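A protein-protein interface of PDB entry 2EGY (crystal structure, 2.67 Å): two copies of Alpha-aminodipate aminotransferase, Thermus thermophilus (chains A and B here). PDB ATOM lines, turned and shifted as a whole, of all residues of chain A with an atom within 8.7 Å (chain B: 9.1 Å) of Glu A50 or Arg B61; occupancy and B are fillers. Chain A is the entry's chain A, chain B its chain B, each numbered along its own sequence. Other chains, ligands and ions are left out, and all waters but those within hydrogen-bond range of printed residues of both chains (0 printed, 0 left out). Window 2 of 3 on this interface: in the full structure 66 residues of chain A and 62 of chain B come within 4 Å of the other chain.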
ATOM      1  N   PHE A  47       1.165 -33.400   0.270  1.00  0.00           N
ATOM      2  CA  PHE A  47       2.271 -32.803   1.032  1.00  0.00           C
ATOM      3  C   PHE A  47       2.167 -32.979   2.541  1.00  0.00           C
ATOM      4  O   PHE A  47       1.238 -32.469   3.169  1.00  0.00           O
ATOM      5  CB  PHE A  47       2.406 -31.309   0.714  1.00  0.00           C
ATOM      6  CG  PHE A  47       2.639 -31.012  -0.743  1.00  0.00           C
ATOM      7  CD1 PHE A  47       3.220 -31.964  -1.582  1.00  0.00           C
ATOM      8  CD2 PHE A  47       2.300 -29.769  -1.271  1.00  0.00           C
ATOM      9  CE1 PHE A  47       3.459 -31.688  -2.919  1.00  0.00           C
ATOM     10  CE2 PHE A  47       2.536 -29.479  -2.608  1.00  0.00           C
ATOM     11  CZ  PHE A  47       3.119 -30.444  -3.437  1.00  0.00           C
ATOM     12  N   PRO A  48       3.145 -33.680   3.142  1.00  0.00           N
ATOM     13  CA  PRO A  48       3.250 -33.978   4.575  1.00  0.00           C
ATOM     14  C   PRO A  48       3.594 -32.746   5.396  1.00  0.00           C
ATOM     15  O   PRO A  48       4.727 -32.587   5.831  1.00  0.00           O
ATOM     16  CB  PRO A  48       4.370 -35.002   4.617  1.00  0.00           C
ATOM     17  CG  PRO A  48       5.303 -34.449   3.592  1.00  0.00           C
ATOM     18  CD  PRO A  48       4.360 -34.136   2.443  1.00  0.00           C
ATOM     19  N   LYS A  49       2.613 -31.884   5.617  1.00  0.00           N
ATOM     20  CA  LYS A  49       2.833 -30.663   6.374  1.00  0.00           C
ATOM     21  C   LYS A  49       3.399 -30.870   7.793  1.00  0.00           C
ATOM     22  O   LYS A  49       4.534 -30.480   8.067  1.00  0.00           O
ATOM     23  CB  LYS A  49       1.525 -29.873   6.431  1.00  0.00           C
ATOM     24  CG  LYS A  49       1.655 -28.458   6.963  1.00  0.00           C
ATOM     25  CD  LYS A  49       0.335 -27.685   6.831  1.00  0.00           C
ATOM     26  CE  LYS A  49       0.035 -27.290   5.384  1.00  0.00           C
ATOM     27  NZ  LYS A  49       0.050 -28.447   4.451  1.00  0.00           N
ATOM     28  N   GLU A  50       2.628 -31.493   8.682  1.00  0.00           N
ATOM     29  CA  GLU A  50       3.062 -31.698  10.070  1.00  0.00           C
ATOM     30  C   GLU A  50       4.233 -32.659  10.284  1.00  0.00           C
ATOM     31  O   GLU A  50       5.017 -32.472  11.213  1.00  0.00           O
ATOM     32  CB  GLU A  50       1.869 -32.137  10.930  1.00  0.00           C
ATOM     33  CG  GLU A  50       2.140 -32.256  12.437  1.00  0.00           C
ATOM     34  CD  GLU A  50       2.575 -30.943  13.090  1.00  0.00           C
ATOM     35  OE1 GLU A  50       2.038 -29.873  12.715  1.00  0.00           O
ATOM     36  OE2 GLU A  50       3.444 -30.991  13.995  1.00  0.00           O
ATOM     37  N   GLU A  51       4.352 -33.690   9.451  1.00  0.00           N
ATOM     38  CA  GLU A  51       5.463 -34.637   9.584  1.00  0.00           C
ATOM     39  C   GLU A  51       6.781 -33.967   9.205  1.00  0.00           C
ATOM     40  O   GLU A  51       7.825 -34.275   9.770  1.00  0.00           O
ATOM     41  CB  GLU A  51       5.268 -35.853   8.682  1.00  0.00           C
ATOM     42  CG  GLU A  51       4.295 -36.895   9.188  1.00  0.00           C
ATOM     43  CD  GLU A  51       4.332 -38.162   8.342  1.00  0.00           C
ATOM     44  OE1 GLU A  51       3.955 -38.096   7.148  1.00  0.00           O
ATOM     45  OE2 GLU A  51       4.748 -39.219   8.869  1.00  0.00           O
ATOM     46  N   ALA A  52       6.724 -33.057   8.238  1.00  0.00           N
ATOM     47  CA  ALA A  52       7.912 -32.344   7.790  1.00  0.00           C
ATOM     48  C   ALA A  52       8.309 -31.279   8.802  1.00  0.00           C
ATOM     49  O   ALA A  52       9.491 -31.071   9.058  1.00  0.00           O
ATOM     50  CB  ALA A  52       7.667 -31.705   6.430  1.00  0.00           C
ATOM     51  N   ALA A  53       7.326 -30.596   9.377  1.00  0.00           N
ATOM     52  CA  ALA A  53       7.626 -29.571  10.368  1.00  0.00           C
ATOM     53  C   ALA A  53       8.298 -30.217  11.575  1.00  0.00           C
ATOM     54  O   ALA A  53       9.082 -29.582  12.262  1.00  0.00           O
ATOM     55  CB  ALA A  53       6.357 -28.853  10.792  1.00  0.00           C
ATOM     56  N   GLU A  54       7.997 -31.485  11.824  1.00  0.00           N
ATOM     57  CA  GLU A  54       8.596 -32.189  12.952  1.00  0.00           C
ATOM     58  C   GLU A  54      10.000 -32.692  12.629  1.00  0.00           C
ATOM     59  O   GLU A  54      10.929 -32.519  13.423  1.00  0.00           O
ATOM     60  CB  GLU A  54       7.709 -33.368  13.382  1.00  0.00           C
ATOM     61  CG  GLU A  54       8.307 -34.252  14.492  1.00  0.00           C
ATOM     62  CD  GLU A  54       9.268 -35.330  13.966  1.00  0.00           C
ATOM     63  OE1 GLU A  54       9.955 -35.989  14.790  1.00  0.00           O
ATOM     64  OE2 GLU A  54       9.323 -35.525  12.727  1.00  0.00           O
ATOM     65  N   ALA A  55      10.149 -33.319  11.466  1.00  0.00           N
ATOM     66  CA  ALA A  55      11.437 -33.850  11.050  1.00  0.00           C
ATOM     67  C   ALA A  55      12.433 -32.717  10.883  1.00  0.00           C
ATOM     68  O   ALA A  55      13.556 -32.800  11.362  1.00  0.00           O
ATOM     69  CB  ALA A  55      11.291 -34.616   9.743  1.00  0.00           C
ATOM     70  N   ALA A  56      12.014 -31.658  10.203  1.00  0.00           N
ATOM     71  CA  ALA A  56      12.877 -30.506   9.969  1.00  0.00           C
ATOM     72  C   ALA A  56      13.345 -29.895  11.291  1.00  0.00           C
ATOM     73  O   ALA A  56      14.551 -29.825  11.566  1.00  0.00           O
ATOM     74  CB  ALA A  56      12.136 -29.464   9.138  1.00  0.00           C
ATOM     75  N   ALA A  57      12.387 -29.457  12.104  1.00  0.00           N
ATOM     76  CA  ALA A  57      12.693 -28.861  13.395  1.00  0.00           C
ATOM     77  C   ALA A  57      13.710 -29.712  14.126  1.00  0.00           C
ATOM     78  O   ALA A  57      14.617 -29.192  14.763  1.00  0.00           O
ATOM     79  CB  ALA A  57      11.430 -28.738  14.227  1.00  0.00           C
ATOM     80  N   ARG A  58      13.569 -31.027  14.025  1.00  0.00           N
ATOM     81  CA  ARG A  58      14.499 -31.935  14.694  1.00  0.00           C
ATOM     82  C   ARG A  58      15.879 -32.003  14.033  1.00  0.00           C
ATOM     83  O   ARG A  58      16.895 -32.129  14.721  1.00  0.00           O
ATOM     84  CB  ARG A  58      13.891 -33.340  14.796  1.00  0.00           C
ATOM     85  CG  ARG A  58      14.848 -34.399  15.306  1.00  0.00           C
ATOM     86  CD  ARG A  58      14.106 -35.597  15.866  1.00  0.00           C
ATOM     87  NE  ARG A  58      12.984 -36.007  15.020  1.00  0.00           N
ATOM     88  CZ  ARG A  58      13.098 -36.443  13.767  1.00  0.00           C
ATOM     89  NH1 ARG A  58      14.295 -36.535  13.195  1.00  0.00           N
ATOM     90  NH2 ARG A  58      12.014 -36.790  13.082  1.00  0.00           N
ATOM     91  N   ARG A  61      17.854 -28.902  15.037  1.00  0.00           N
ATOM     92  CA  ARG A  61      18.220 -28.974  16.457  1.00  0.00           C
ATOM     93  C   ARG A  61      19.291 -30.000  16.793  1.00  0.00           C
ATOM     94  O   ARG A  61      20.354 -29.657  17.306  1.00  0.00           O
ATOM     95  CB  ARG A  61      16.986 -29.258  17.311  1.00  0.00           C
ATOM     96  CG  ARG A  61      16.151 -28.025  17.584  1.00  0.00           C
ATOM     97  CD  ARG A  61      14.787 -28.375  18.144  1.00  0.00           C
ATOM     98  NE  ARG A  61      13.941 -27.188  18.214  1.00  0.00           N
ATOM     99  CZ  ARG A  61      12.627 -27.195  18.014  1.00  0.00           C
ATOM    100  NH1 ARG A  61      12.010 -28.336  17.734  1.00  0.00           N
ATOM    101  NH2 ARG A  61      11.936 -26.064  18.085  1.00  0.00           N
ATOM    102  N   LEU A 277      15.839 -33.959   5.243  1.00  0.00           N
ATOM    103  CA  LEU A 277      14.411 -33.902   5.510  1.00  0.00           C
ATOM    104  C   LEU A 277      13.697 -34.987   4.701  1.00  0.00           C
ATOM    105  O   LEU A 277      12.921 -35.766   5.244  1.00  0.00           O
ATOM    106  CB  LEU A 277      13.846 -32.511   5.179  1.00  0.00           C
ATOM    107  CG  LEU A 277      12.317 -32.387   5.144  1.00  0.00           C
ATOM    108  CD1 LEU A 277      11.705 -33.061   6.357  1.00  0.00           C
ATOM    109  CD2 LEU A 277      11.926 -30.919   5.087  1.00  0.00           C
ATOM    110  N   LEU A 281      11.549 -38.215   6.166  1.00  0.00           N
ATOM    111  CA  LEU A 281      10.163 -38.494   5.842  1.00  0.00           C
ATOM    112  C   LEU A 281       9.942 -39.811   5.119  1.00  0.00           C
ATOM    113  O   LEU A 281       8.839 -40.339   5.140  1.00  0.00           O
ATOM    114  CB  LEU A 281       9.578 -37.364   4.999  1.00  0.00           C
ATOM    115  CG  LEU A 281       9.440 -36.012   5.695  1.00  0.00           C
ATOM    116  CD1 LEU A 281       8.912 -34.977   4.729  1.00  0.00           C
ATOM    117  CD2 LEU A 281       8.497 -36.152   6.875  1.00  0.00           C
ATOM    118  N   ARG A 289       2.568 -44.266   1.692  1.00  0.00           N
ATOM    119  CA  ARG A 289       2.539 -42.936   1.092  1.00  0.00           C
ATOM    120  C   ARG A 289       2.339 -43.065  -0.410  1.00  0.00           C
ATOM    121  O   ARG A 289       1.512 -42.367  -0.990  1.00  0.00           O
ATOM    122  CB  ARG A 289       3.840 -42.187   1.369  1.00  0.00           C
ATOM    123  CG  ARG A 289       4.013 -40.920   0.545  1.00  0.00           C
ATOM    124  CD  ARG A 289       5.281 -40.206   0.948  1.00  0.00           C
ATOM    125  NE  ARG A 289       5.186 -39.791   2.337  1.00  0.00           N
ATOM    126  CZ  ARG A 289       4.404 -38.802   2.754  1.00  0.00           C
ATOM    127  NH1 ARG A 289       3.666 -38.131   1.873  1.00  0.00           N
ATOM    128  NH2 ARG A 289       4.332 -38.507   4.047  1.00  0.00           N
ATOM    129  N   ALA B  53      15.434 -24.135  13.508  1.00  0.00           N
ATOM    130  CA  ALA B  53      14.542 -25.254  13.760  1.00  0.00           C
ATOM    131  C   ALA B  53      13.143 -24.709  14.013  1.00  0.00           C
ATOM    132  O   ALA B  53      12.155 -25.234  13.498  1.00  0.00           O
ATOM    133  CB  ALA B  53      15.025 -26.042  14.971  1.00  0.00           C
ATOM    134  N   GLU B  54      13.072 -23.647  14.811  1.00  0.00           N
ATOM    135  CA  GLU B  54      11.799 -23.015  15.138  1.00  0.00           C
ATOM    136  C   GLU B  54      11.162 -22.403  13.901  1.00  0.00           C
ATOM    137  O   GLU B  54       9.998 -22.648  13.615  1.00  0.00           O
ATOM    138  CB  GLU B  54      12.004 -21.939  16.207  1.00  0.00           C
ATOM    139  CG  GLU B  54      10.731 -21.207  16.605  1.00  0.00           C
ATOM    140  CD  GLU B  54      10.387 -20.071  15.657  1.00  0.00           C
ATOM    141  OE1 GLU B  54       9.186 -19.740  15.539  1.00  0.00           O
ATOM    142  OE2 GLU B  54      11.317 -19.501  15.041  1.00  0.00           O
ATOM    143  N   ALA B  55      11.934 -21.618  13.159  1.00  0.00           N
ATOM    144  CA  ALA B  55      11.420 -20.976  11.952  1.00  0.00           C
ATOM    145  C   ALA B  55      11.029 -21.984  10.881  1.00  0.00           C
ATOM    146  O   ALA B  55      10.096 -21.753  10.120  1.00  0.00           O
ATOM    147  CB  ALA B  55      12.449 -20.005  11.401  1.00  0.00           C
ATOM    148  N   ALA B  56      11.745 -23.098  10.818  1.00  0.00           N
ATOM    149  CA  ALA B  56      11.452 -24.124   9.827  1.00  0.00           C
ATOM    150  C   ALA B  56      10.106 -24.781  10.109  1.00  0.00           C
ATOM    151  O   ALA B  56       9.292 -24.947   9.205  1.00  0.00           O
ATOM    152  CB  ALA B  56      12.561 -25.179   9.809  1.00  0.00           C
ATOM    153  N   ALA B  57       9.872 -25.154  11.363  1.00  0.00           N
ATOM    154  CA  ALA B  57       8.614 -25.796  11.749  1.00  0.00           C
ATOM    155  C   ALA B  57       7.434 -24.838  11.565  1.00  0.00           C
ATOM    156  O   ALA B  57       6.418 -25.183  10.964  1.00  0.00           O
ATOM    157  CB  ALA B  57       8.692 -26.263  13.196  1.00  0.00           C
ATOM    158  N   ARG B  58       7.579 -23.631  12.092  1.00  0.00           N
ATOM    159  CA  ARG B  58       6.543 -22.617  11.983  1.00  0.00           C
ATOM    160  C   ARG B  58       6.175 -22.448  10.513  1.00  0.00           C
ATOM    161  O   ARG B  58       5.002 -22.346  10.163  1.00  0.00           O
ATOM    162  CB  ARG B  58       7.069 -21.303  12.570  1.00  0.00           C
ATOM    163  CG  ARG B  58       6.281 -20.065  12.204  1.00  0.00           C
ATOM    164  CD  ARG B  58       7.179 -18.849  12.304  1.00  0.00           C
ATOM    165  NE  ARG B  58       7.432 -18.480  13.689  1.00  0.00           N
ATOM    166  CZ  ARG B  58       6.584 -17.776  14.436  1.00  0.00           C
ATOM    167  NH1 ARG B  58       5.427 -17.364  13.923  1.00  0.00           N
ATOM    168  NH2 ARG B  58       6.892 -17.469  15.692  1.00  0.00           N
ATOM    169  N   ILE B  59       7.192 -22.437   9.658  1.00  0.00           N
ATOM    170  CA  ILE B  59       7.011 -22.272   8.220  1.00  0.00           C
ATOM    171  C   ILE B  59       6.313 -23.453   7.570  1.00  0.00           C
ATOM    172  O   ILE B  59       5.339 -23.277   6.850  1.00  0.00           O
ATOM    173  CB  ILE B  59       8.368 -22.062   7.501  1.00  0.00           C
ATOM    174  CG1 ILE B  59       8.888 -20.651   7.769  1.00  0.00           C
ATOM    175  CG2 ILE B  59       8.216 -22.292   6.005  1.00  0.00           C
ATOM    176  CD1 ILE B  59      10.153 -20.314   7.016  1.00  0.00           C
ATOM    177  N   LEU B  60       6.823 -24.653   7.815  1.00  0.00           N
ATOM    178  CA  LEU B  60       6.248 -25.859   7.231  1.00  0.00           C
ATOM    179  C   LEU B  60       4.847 -26.134   7.736  1.00  0.00           C
ATOM    180  O   LEU B  60       3.989 -26.589   6.992  1.00  0.00           O
ATOM    181  CB  LEU B  60       7.142 -27.064   7.529  1.00  0.00           C
ATOM    182  CG  LEU B  60       8.414 -27.134   6.686  1.00  0.00           C
ATOM    183  CD1 LEU B  60       9.308 -28.246   7.190  1.00  0.00           C
ATOM    184  CD2 LEU B  60       8.037 -27.356   5.229  1.00  0.00           C
ATOM    185  N   ARG B  61       4.627 -25.845   9.012  1.00  0.00           N
ATOM    186  CA  ARG B  61       3.341 -26.066   9.659  1.00  0.00           C
ATOM    187  C   ARG B  61       2.286 -25.039   9.235  1.00  0.00           C
ATOM    188  O   ARG B  61       1.154 -25.403   8.934  1.00  0.00           O
ATOM    189  CB  ARG B  61       3.540 -26.043  11.179  1.00  0.00           C
ATOM    190  CG  ARG B  61       2.388 -26.630  11.993  1.00  0.00           C
ATOM    191  CD  ARG B  61       2.741 -26.670  13.478  1.00  0.00           C
ATOM    192  NE  ARG B  61       3.712 -27.716  13.803  1.00  0.00           N
ATOM    193  CZ  ARG B  61       4.717 -27.564  14.664  1.00  0.00           C
ATOM    194  NH1 ARG B  61       4.891 -26.405  15.287  1.00  0.00           N
ATOM    195  NH2 ARG B  61       5.545 -28.575  14.907  1.00  0.00           N
ATOM    196  N   GLU B  62       2.667 -23.765   9.194  1.00  0.00           N
ATOM    197  CA  GLU B  62       1.754 -22.682   8.821  1.00  0.00           C
ATOM    198  C   GLU B  62       1.636 -22.379   7.322  1.00  0.00           C
ATOM    199  O   GLU B  62       0.673 -21.743   6.895  1.00  0.00           O
ATOM    200  CB  GLU B  62       2.156 -21.389   9.532  1.00  0.00           C
ATOM    201  CG  GLU B  62       2.034 -21.412  11.047  1.00  0.00           C
ATOM    202  CD  GLU B  62       2.433 -20.081  11.672  1.00  0.00           C
ATOM    203  OE1 GLU B  62       2.301 -19.932  12.905  1.00  0.00           O
ATOM    204  OE2 GLU B  62       2.884 -19.183  10.924  1.00  0.00           O
ATOM    205  N   LYS B  63       2.607 -22.816   6.527  1.00  0.00           N
ATOM    206  CA  LYS B  63       2.584 -22.553   5.089  1.00  0.00           C
ATOM    207  C   LYS B  63       3.186 -23.692   4.270  1.00  0.00           C
ATOM    208  O   LYS B  63       3.798 -23.451   3.232  1.00  0.00           O
ATOM    209  CB  LYS B  63       3.364 -21.274   4.783  1.00  0.00           C
ATOM    210  CG  LYS B  63       2.944 -20.055   5.582  1.00  0.00           C
ATOM    211  CD  LYS B  63       3.747 -18.837   5.150  1.00  0.00           C
ATOM    212  CE  LYS B  63       3.288 -17.575   5.862  1.00  0.00           C
ATOM    213  NZ  LYS B  63       3.997 -16.362   5.366  1.00  0.00           N
ATOM    214  N   GLY B  64       3.004 -24.927   4.728  1.00  0.00           N
ATOM    215  CA  GLY B  64       3.567 -26.075   4.029  1.00  0.00           C
ATOM    216  C   GLY B  64       3.172 -26.314   2.579  1.00  0.00           C
ATOM    217  O   GLY B  64       3.910 -26.970   1.835  1.00  0.00           O
ATOM    218  N   GLU B  65       2.011 -25.793   2.183  1.00  0.00           N
ATOM    219  CA  GLU B  65       1.492 -25.947   0.825  1.00  0.00           C
ATOM    220  C   GLU B  65       2.089 -24.892  -0.098  1.00  0.00           C
ATOM    221  O   GLU B  65       1.576 -24.636  -1.184  1.00  0.00           O
ATOM    222  CB  GLU B  65      -0.037 -25.809   0.827  1.00  0.00           C
ATOM    223  CG  GLU B  65      -0.553 -24.383   1.137  1.00  0.00           C
ATOM    224  CD  GLU B  65      -0.172 -23.876   2.537  1.00  0.00           C
ATOM    225  OE1 GLU B  65       0.360 -22.742   2.635  1.00  0.00           O
ATOM    226  OE2 GLU B  65      -0.410 -24.601   3.533  1.00  0.00           O
ATOM    227  N   VAL B  66       3.164 -24.262   0.348  1.00  0.00           N
ATOM    228  CA  VAL B  66       3.824 -23.237  -0.443  1.00  0.00           C
ATOM    229  C   VAL B  66       5.307 -23.564  -0.447  1.00  0.00           C
ATOM    230  O   VAL B  66       5.976 -23.477  -1.480  1.00  0.00           O
ATOM    231  CB  VAL B  66       3.586 -21.823   0.159  1.00  0.00           C
ATOM    232  CG1 VAL B  66       4.443 -20.793  -0.533  1.00  0.00           C
ATOM    233  CG2 VAL B  66       2.135 -21.442   0.006  1.00  0.00           C
ATOM    234  N   ALA B  67       5.811 -23.959   0.714  1.00  0.00           N
ATOM    235  CA  ALA B  67       7.214 -24.306   0.857  1.00  0.00           C
ATOM    236  C   ALA B  67       7.525 -25.620   0.137  1.00  0.00           C
ATOM    237  O   ALA B  67       8.642 -25.831  -0.333  1.00  0.00           O
ATOM    238  CB  ALA B  67       7.563 -24.421   2.335  1.00  0.00           C
ATOM    239  N   LEU B  68       6.524 -26.491   0.048  1.00  0.00           N
ATOM    240  CA  LEU B  68       6.667 -27.793  -0.598  1.00  0.00           C
ATOM    241  C   LEU B  68       6.141 -27.862  -2.042  1.00  0.00           C
ATOM    242  O   LEU B  68       6.265 -28.888  -2.706  1.00  0.00           O
ATOM    243  CB  LEU B  68       5.960 -28.850   0.251  1.00  0.00           C
ATOM    244  CG  LEU B  68       6.723 -29.531   1.382  1.00  0.00           C
ATOM    245  CD1 LEU B  68       7.780 -28.625   1.970  1.00  0.00           C
ATOM    246  CD2 LEU B  68       5.722 -29.962   2.419  1.00  0.00           C
ATOM    247  N   LEU B 273      11.565 -23.737   0.901  1.00  0.00           N
ATOM    248  CA  LEU B 273      11.822 -23.775   2.333  1.00  0.00           C
ATOM    249  C   LEU B 273      13.044 -22.902   2.596  1.00  0.00           C
ATOM    250  O   LEU B 273      12.976 -21.893   3.293  1.00  0.00           O
ATOM    251  CB  LEU B 273      12.134 -25.206   2.790  1.00  0.00           C
ATOM    252  CG  LEU B 273      11.545 -25.750   4.102  1.00  0.00           C
ATOM    253  CD1 LEU B 273      12.456 -26.855   4.612  1.00  0.00           C
ATOM    254  CD2 LEU B 273      11.405 -24.651   5.153  1.00  0.00           C
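Glu A50 touches one residue of chain B. Printed residues of chain B within 4 Å of Ala A52: Leu B60. Printed residues of chain B within 4 Å of Ala A53: Ala B57 (3.5 Å), Leu B60 (3.8 Å) and Arg B61 (3.9 Å). Of chain A, only Lys A49, Glu A50 and Ala A53 come within 4 Å of Arg B61. Lys B63 touches none of the printed residues of chain A. Of the printed residues of chain A, Leu B68 touches Phe A47. The nearest residue of chain B that does not touch Glu A50 is Leu B60 (5.4 Å). The nearest residue of chain A that does not touch Arg B61 is Glu A54 (4.9 Å). The nearest printed residue of chain A that does not touch Ala B57 is Ala A56 (5.4 Å).
The side-chain carboxylate (OE2) of Glu B65 lies within salt-bridge range of the side-chain amino group (NZ) of Lys A49. NE of Arg B61 is in salt-bridge range of OE1 of Glu A50 (2.9 Å).
Printed residues of chain A that touch a printed residue of chain B: Phe A47, Lys A49, Glu A50, Ala A52, Ala A53, Ala A56, Ala A57 and Arg A61. Along chain A the printed residues that touch a printed residue of chain B span positions 47 to 61. Hydrophobic or aromatic side chains of chain B that line the printed part of chain A: Ala B53, Ala B57, Leu B60 and Leu B68. Among the printed residues, Asp or Glu carboxylates within 4 Å of a Lys or Arg side-chain nitrogen of the other chain: Lys A49 with Glu B65 and Glu A50 with Arg B61.
Ala A53 touches Ala B57, and with the chains exchanged Ala A57 touches Ala B53. Ala A53 touches Arg B61, and with the chains exchanged Arg A61 touches Ala B53. Ala A57 touches its own counterpart, Ala B57. 7 positions are printed for both chains. Of the 14 pairs that touch across the chains among the printed residues, 5 have their exchanged pair printed and touching as well.
Lys A49 touches Leu B60 (CG to O, 3.0 Å). Arg B61 touches Lys A49 (O to CD, 3.2 Å). Lys A49 touches Gly B64 (CE to N, 3.9 Å). O of Ala A52 touches CD1 of Leu B60, at 3.4 Å. Ala A53 touches Ala B57. Arg B61 touches Ala A53 (N to CB, 3.9 Å). Leu B60 touches Ala A56. Ala A57 touches Ala B53. Ala A57 touches Ala B57 (CB to CB, 3.8 Å). Arg A61 touches Ala B53.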
